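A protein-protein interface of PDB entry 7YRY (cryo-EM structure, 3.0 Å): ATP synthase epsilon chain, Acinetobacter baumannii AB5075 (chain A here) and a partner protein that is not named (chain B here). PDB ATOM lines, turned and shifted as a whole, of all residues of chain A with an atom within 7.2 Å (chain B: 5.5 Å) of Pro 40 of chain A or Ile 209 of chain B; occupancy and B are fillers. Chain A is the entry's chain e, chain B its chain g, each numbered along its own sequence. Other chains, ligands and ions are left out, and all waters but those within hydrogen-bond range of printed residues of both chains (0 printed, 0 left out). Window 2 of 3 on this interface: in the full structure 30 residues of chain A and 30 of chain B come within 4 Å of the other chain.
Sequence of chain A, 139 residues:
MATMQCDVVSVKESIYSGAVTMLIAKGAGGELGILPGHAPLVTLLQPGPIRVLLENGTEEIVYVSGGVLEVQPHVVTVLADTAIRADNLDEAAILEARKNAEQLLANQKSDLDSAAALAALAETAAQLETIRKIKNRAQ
The backbone carbonyl oxygen (O) of Tyr 208 of chain B lies close to the side-chain hydroxyl (OH) of Tyr 210 of chain B (3.3 Å).
The backbone NH (N) of Leu 69 of chain A lies within hydrogen-bond range of the backbone carbonyl oxygen (O) of Thr 43 of chain A, at 2.4 Å.
OE2 of Glu 211 of chain B sits close to O of Val 42 of chain A (3.2 Å).
O of Pro 40 of chain A sits at hydrogen-bond distance from N of Ile 209 of chain B (3.3 Å).
The side-chain carboxylate (OE1) of Glu 211 of chain B is in hydrogen-bond range of the side-chain hydroxyl (OG1) of Thr 43 of chain A, at 2.8 Å.
Pro 40 of chain A touches two residues of chain B.
Ile 209 of chain B touches three residues of chain A.
Of the printed residues of chain B, Thr 43 of chain A touches Glu 211.
Of the printed residues of chain A, Tyr 208 of chain B touches Pro 40 (3.7 Å) and Glu 70 (3.9 Å).
Gly 37 of chain A touches none of the printed residues of chain B.
The nearest residue of chain A that does not touch Ile 209 of chain B is Ala 39 of chain A (5.0 Å).
Printed residues of chain A that touch a printed residue of chain B: Pro 40, Leu 41, Val 42, Thr 43 and Glu 70.
Hydrophobic or aromatic side chains of chain A within 4 Å of the printed part of chain B: Leu 41 and Val 42.
Along chain A the printed residues that touch a printed residue of chain B span positions 40 to 70.
Of the 5 printed residues of chain B, 4 touch a printed residue of chain A.
Hydrophobic or aromatic side chains of chain B that line the printed part of chain A: Tyr 208, Ile 209 and Tyr 210.
Along chain B the printed residues that touch a printed residue of chain A span positions 208 to 211.
Among the printed residues, 8 pairs touch across the chains.
Among the printed residues, pairs that only touch across the chains: Pro 40 of chain A with Tyr 208 of chain B, Leu 41 of chain A with Ile 209 of chain B, Val 42 of chain A with Ile 209 of chain B, Val 42 of chain A with Tyr 210 of chain B and Glu 70 of chain A with Tyr 208 of chain B.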
ATOM      1  N   GLY A  37       7.879 -12.688  19.969  1.00  0.00           N
ATOM      2  CA  GLY A  37       7.955 -11.301  20.373  1.00  0.00           C
ATOM      3  C   GLY A  37       7.441 -10.305  19.358  1.00  0.00           C
ATOM      4  O   GLY A  37       7.614  -9.098  19.558  1.00  0.00           O
ATOM      5  N   HIS A  38       6.820 -10.769  18.277  1.00  0.00           N
ATOM      6  CA  HIS A  38       6.318  -9.869  17.249  1.00  0.00           C
ATOM      7  C   HIS A  38       5.140  -9.050  17.768  1.00  0.00           C
ATOM      8  O   HIS A  38       4.381  -9.488  18.638  1.00  0.00           O
ATOM      9  CB  HIS A  38       5.900 -10.661  16.011  1.00  0.00           C
ATOM     10  CG  HIS A  38       5.626  -9.811  14.809  1.00  0.00           C
ATOM     11  ND1 HIS A  38       4.430  -9.153  14.619  1.00  0.00           N
ATOM     12  CD2 HIS A  38       6.393  -9.515  13.734  1.00  0.00           C
ATOM     13  CE1 HIS A  38       4.473  -8.485  13.480  1.00  0.00           C
ATOM     14  NE2 HIS A  38       5.653  -8.689  12.923  1.00  0.00           N
ATOM     15  N   ALA A  39       5.000  -7.845  17.228  1.00  0.00           N
ATOM     16  CA  ALA A  39       3.867  -6.997  17.578  1.00  0.00           C
ATOM     17  C   ALA A  39       2.574  -7.622  17.063  1.00  0.00           C
ATOM     18  O   ALA A  39       2.507  -8.018  15.894  1.00  0.00           O
ATOM     19  CB  ALA A  39       4.047  -5.596  16.998  1.00  0.00           C
ATOM     20  N   PRO A  40       1.541  -7.738  17.896  1.00  0.00           N
ATOM     21  CA  PRO A  40       0.296  -8.368  17.442  1.00  0.00           C
ATOM     22  C   PRO A  40      -0.367  -7.571  16.328  1.00  0.00           C
ATOM     23  O   PRO A  40      -0.282  -6.342  16.275  1.00  0.00           O
ATOM     24  CB  PRO A  40      -0.576  -8.390  18.704  1.00  0.00           C
ATOM     25  CG  PRO A  40       0.387  -8.235  19.842  1.00  0.00           C
ATOM     26  CD  PRO A  40       1.489  -7.371  19.320  1.00  0.00           C
ATOM     27  N   LEU A  41      -1.039  -8.290  15.433  1.00  0.00           N
ATOM     28  CA  LEU A  41      -1.709  -7.663  14.303  1.00  0.00           C
ATOM     29  C   LEU A  41      -2.764  -8.616  13.762  1.00  0.00           C
ATOM     30  O   LEU A  41      -2.761  -9.814  14.052  1.00  0.00           O
ATOM     31  CB  LEU A  41      -0.716  -7.276  13.199  1.00  0.00           C
ATOM     32  CG  LEU A  41      -0.042  -8.371  12.366  1.00  0.00           C
ATOM     33  CD1 LEU A  41       0.594  -7.761  11.129  1.00  0.00           C
ATOM     34  CD2 LEU A  41       1.003  -9.128  13.168  1.00  0.00           C
ATOM     35  N   VAL A  42      -3.671  -8.058  12.966  1.00  0.00           N
ATOM     36  CA  VAL A  42      -4.672  -8.822  12.235  1.00  0.00           C
ATOM     37  C   VAL A  42      -4.531  -8.485  10.759  1.00  0.00           C
ATOM     38  O   VAL A  42      -4.425  -7.310  10.390  1.00  0.00           O
ATOM     39  CB  VAL A  42      -6.104  -8.527  12.731  1.00  0.00           C
ATOM     40  CG1 VAL A  42      -6.421  -9.341  13.975  1.00  0.00           C
ATOM     41  CG2 VAL A  42      -6.274  -7.054  13.010  1.00  0.00           C
ATOM     42  N   THR A  43      -4.522  -9.513   9.913  1.00  0.00           N
ATOM     43  CA  THR A  43      -4.254  -9.307   8.497  1.00  0.00           C
ATOM     44  C   THR A  43      -5.074 -10.283   7.668  1.00  0.00           C
ATOM     45  O   THR A  43      -5.154 -11.471   7.991  1.00  0.00           O
ATOM     46  CB  THR A  43      -2.761  -9.478   8.188  1.00  0.00           C
ATOM     47  OG1 THR A  43      -2.007  -8.496   8.909  1.00  0.00           O
ATOM     48  CG2 THR A  43      -2.495  -9.318   6.697  1.00  0.00           C
ATOM     49  N   LEU A  69      -5.787 -12.903   9.829  1.00  0.00           N
ATOM     50  CA  LEU A  69      -4.728 -13.414  10.685  1.00  0.00           C
ATOM     51  C   LEU A  69      -4.861 -12.831  12.088  1.00  0.00           C
ATOM     52  O   LEU A  69      -5.508 -11.803  12.293  1.00  0.00           O
ATOM     53  CB  LEU A  69      -3.366 -13.062  10.073  1.00  0.00           C
ATOM     54  CG  LEU A  69      -1.987 -13.318  10.697  1.00  0.00           C
ATOM     55  CD1 LEU A  69      -1.584 -12.180  11.630  1.00  0.00           C
ATOM     56  CD2 LEU A  69      -1.882 -14.673  11.387  1.00  0.00           C
ATOM     57  N   GLU A  70      -4.265 -13.520  13.060  1.00  0.00           N
ATOM     58  CA  GLU A  70      -4.120 -12.988  14.414  1.00  0.00           C
ATOM     59  C   GLU A  70      -2.966 -13.727  15.079  1.00  0.00           C
ATOM     60  O   GLU A  70      -3.107 -14.897  15.445  1.00  0.00           O
ATOM     61  CB  GLU A  70      -5.409 -13.140  15.217  1.00  0.00           C
ATOM     62  CG  GLU A  70      -5.366 -12.537  16.623  1.00  0.00           C
ATOM     63  CD  GLU A  70      -4.315 -11.451  16.784  1.00  0.00           C
ATOM     64  OE1 GLU A  70      -4.557 -10.310  16.341  1.00  0.00           O
ATOM     65  OE2 GLU A  70      -3.243 -11.740  17.358  1.00  0.00           O
ATOM     66  N   VAL A  71      -1.836 -13.045  15.240  1.00  0.00           N
ATOM     67  CA  VAL A  71      -0.655 -13.623  15.871  1.00  0.00           C
ATOM     68  C   VAL A  71      -0.173 -12.673  16.957  1.00  0.00           C
ATOM     69  O   VAL A  71      -0.184 -11.451  16.780  1.00  0.00           O
ATOM     70  CB  VAL A  71       0.463 -13.907  14.844  1.00  0.00           C
ATOM     71  CG1 VAL A  71       0.890 -12.631  14.142  1.00  0.00           C
ATOM     72  CG2 VAL A  71       1.655 -14.574  15.515  1.00  0.00           C
ATOM     73  N   GLN A  72       0.230 -13.239  18.092  1.00  0.00           N
ATOM     74  CA  GLN A  72       0.793 -12.464  19.187  1.00  0.00           C
ATOM     75  C   GLN A  72       1.674 -13.392  20.008  1.00  0.00           C
ATOM     76  O   GLN A  72       1.482 -14.612  19.962  1.00  0.00           O
ATOM     77  CB  GLN A  72      -0.318 -11.824  20.040  1.00  0.00           C
ATOM     78  CG  GLN A  72      -1.147 -12.762  20.901  1.00  0.00           C
ATOM     79  CD  GLN A  72      -0.608 -12.895  22.310  1.00  0.00           C
ATOM     80  OE1 GLN A  72       0.372 -12.249  22.678  1.00  0.00           O
ATOM     81  NE2 GLN A  72      -1.279 -13.699  23.122  1.00  0.00           N
ATOM     82  N   PRO A  73       2.651 -12.859  20.750  1.00  0.00           N
ATOM     83  CA  PRO A  73       3.698 -13.730  21.317  1.00  0.00           C
ATOM     84  C   PRO A  73       3.192 -14.849  22.215  1.00  0.00           C
ATOM     85  O   PRO A  73       3.889 -15.860  22.368  1.00  0.00           O
ATOM     86  CB  PRO A  73       4.587 -12.742  22.091  1.00  0.00           C
ATOM     87  CG  PRO A  73       3.759 -11.502  22.248  1.00  0.00           C
ATOM     88  CD  PRO A  73       2.941 -11.438  21.004  1.00  0.00           C
ATOM     89  N   ASP B 207      -2.689  -2.239  21.859  1.00  0.00           N
ATOM     90  CA  ASP B 207      -3.639  -2.380  20.766  1.00  0.00           C
ATOM     91  C   ASP B 207      -2.951  -3.067  19.597  1.00  0.00           C
ATOM     92  O   ASP B 207      -1.753  -2.879  19.369  1.00  0.00           O
ATOM     93  CB  ASP B 207      -4.194  -1.021  20.319  1.00  0.00           C
ATOM     94  CG  ASP B 207      -5.348  -0.549  21.178  1.00  0.00           C
ATOM     95  OD1 ASP B 207      -6.072  -1.404  21.724  1.00  0.00           O
ATOM     96  OD2 ASP B 207      -5.529   0.680  21.308  1.00  0.00           O
ATOM     97  N   TYR B 208      -3.716  -3.865  18.855  1.00  0.00           N
ATOM     98  CA  TYR B 208      -3.180  -4.462  17.643  1.00  0.00           C
ATOM     99  C   TYR B 208      -2.969  -3.395  16.573  1.00  0.00           C
ATOM    100  O   TYR B 208      -3.569  -2.316  16.602  1.00  0.00           O
ATOM    101  CB  TYR B 208      -4.105  -5.553  17.097  1.00  0.00           C
ATOM    102  CG  TYR B 208      -4.948  -6.272  18.126  1.00  0.00           C
ATOM    103  CD1 TYR B 208      -4.442  -7.359  18.827  1.00  0.00           C
ATOM    104  CD2 TYR B 208      -6.257  -5.885  18.375  1.00  0.00           C
ATOM    105  CE1 TYR B 208      -5.211  -8.029  19.760  1.00  0.00           C
ATOM    106  CE2 TYR B 208      -7.034  -6.550  19.303  1.00  0.00           C
ATOM    107  CZ  TYR B 208      -6.505  -7.617  19.997  1.00  0.00           C
ATOM    108  OH  TYR B 208      -7.279  -8.279  20.924  1.00  0.00           O
ATOM    109  N   ILE B 209      -2.102  -3.711  15.617  1.00  0.00           N
ATOM    110  CA  ILE B 209      -1.823  -2.841  14.482  1.00  0.00           C
ATOM    111  C   ILE B 209      -2.477  -3.448  13.247  1.00  0.00           C
ATOM    112  O   ILE B 209      -2.553  -4.675  13.112  1.00  0.00           O
ATOM    113  CB  ILE B 209      -0.308  -2.634  14.280  1.00  0.00           C
ATOM    114  CG1 ILE B 209      -0.044  -1.528  13.254  1.00  0.00           C
ATOM    115  CG2 ILE B 209       0.379  -3.933  13.882  1.00  0.00           C
ATOM    116  CD1 ILE B 209       1.331  -0.909  13.364  1.00  0.00           C
ATOM    117  N   TYR B 210      -2.976  -2.587  12.364  1.00  0.00           N
ATOM    118  CA  TYR B 210      -3.748  -3.015  11.203  1.00  0.00           C
ATOM    119  C   TYR B 210      -3.209  -2.304   9.972  1.00  0.00           C
ATOM    120  O   TYR B 210      -3.235  -1.071   9.909  1.00  0.00           O
ATOM    121  CB  TYR B 210      -5.234  -2.694  11.389  1.00  0.00           C
ATOM    122  CG  TYR B 210      -5.673  -2.620  12.835  1.00  0.00           C
ATOM    123  CD1 TYR B 210      -5.831  -3.769  13.594  1.00  0.00           C
ATOM    124  CD2 TYR B 210      -5.929  -1.397  13.441  1.00  0.00           C
ATOM    125  CE1 TYR B 210      -6.231  -3.706  14.915  1.00  0.00           C
ATOM    126  CE2 TYR B 210      -6.330  -1.323  14.762  1.00  0.00           C
ATOM    127  CZ  TYR B 210      -6.479  -2.481  15.493  1.00  0.00           C
ATOM    128  OH  TYR B 210      -6.877  -2.416  16.808  1.00  0.00           O
ATOM    129  N   GLU B 211      -2.715  -3.073   9.002  1.00  0.00           N
ATOM    130  CA  GLU B 211      -2.272  -2.456   7.754  1.00  0.00           C
ATOM    131  C   GLU B 211      -3.401  -1.755   6.997  1.00  0.00           C
ATOM    132  O   GLU B 211      -3.152  -0.657   6.469  1.00  0.00           O
ATOM    133  CB  GLU B 211      -1.522  -3.473   6.871  1.00  0.00           C
ATOM    134  CG  GLU B 211      -2.259  -4.725   6.407  1.00  0.00           C
ATOM    135  CD  GLU B 211      -2.569  -5.694   7.530  1.00  0.00           C
ATOM    136  OE1 GLU B 211      -1.774  -5.774   8.490  1.00  0.00           O
ATOM    137  OE2 GLU B 211      -3.615  -6.371   7.455  1.00  0.00           O
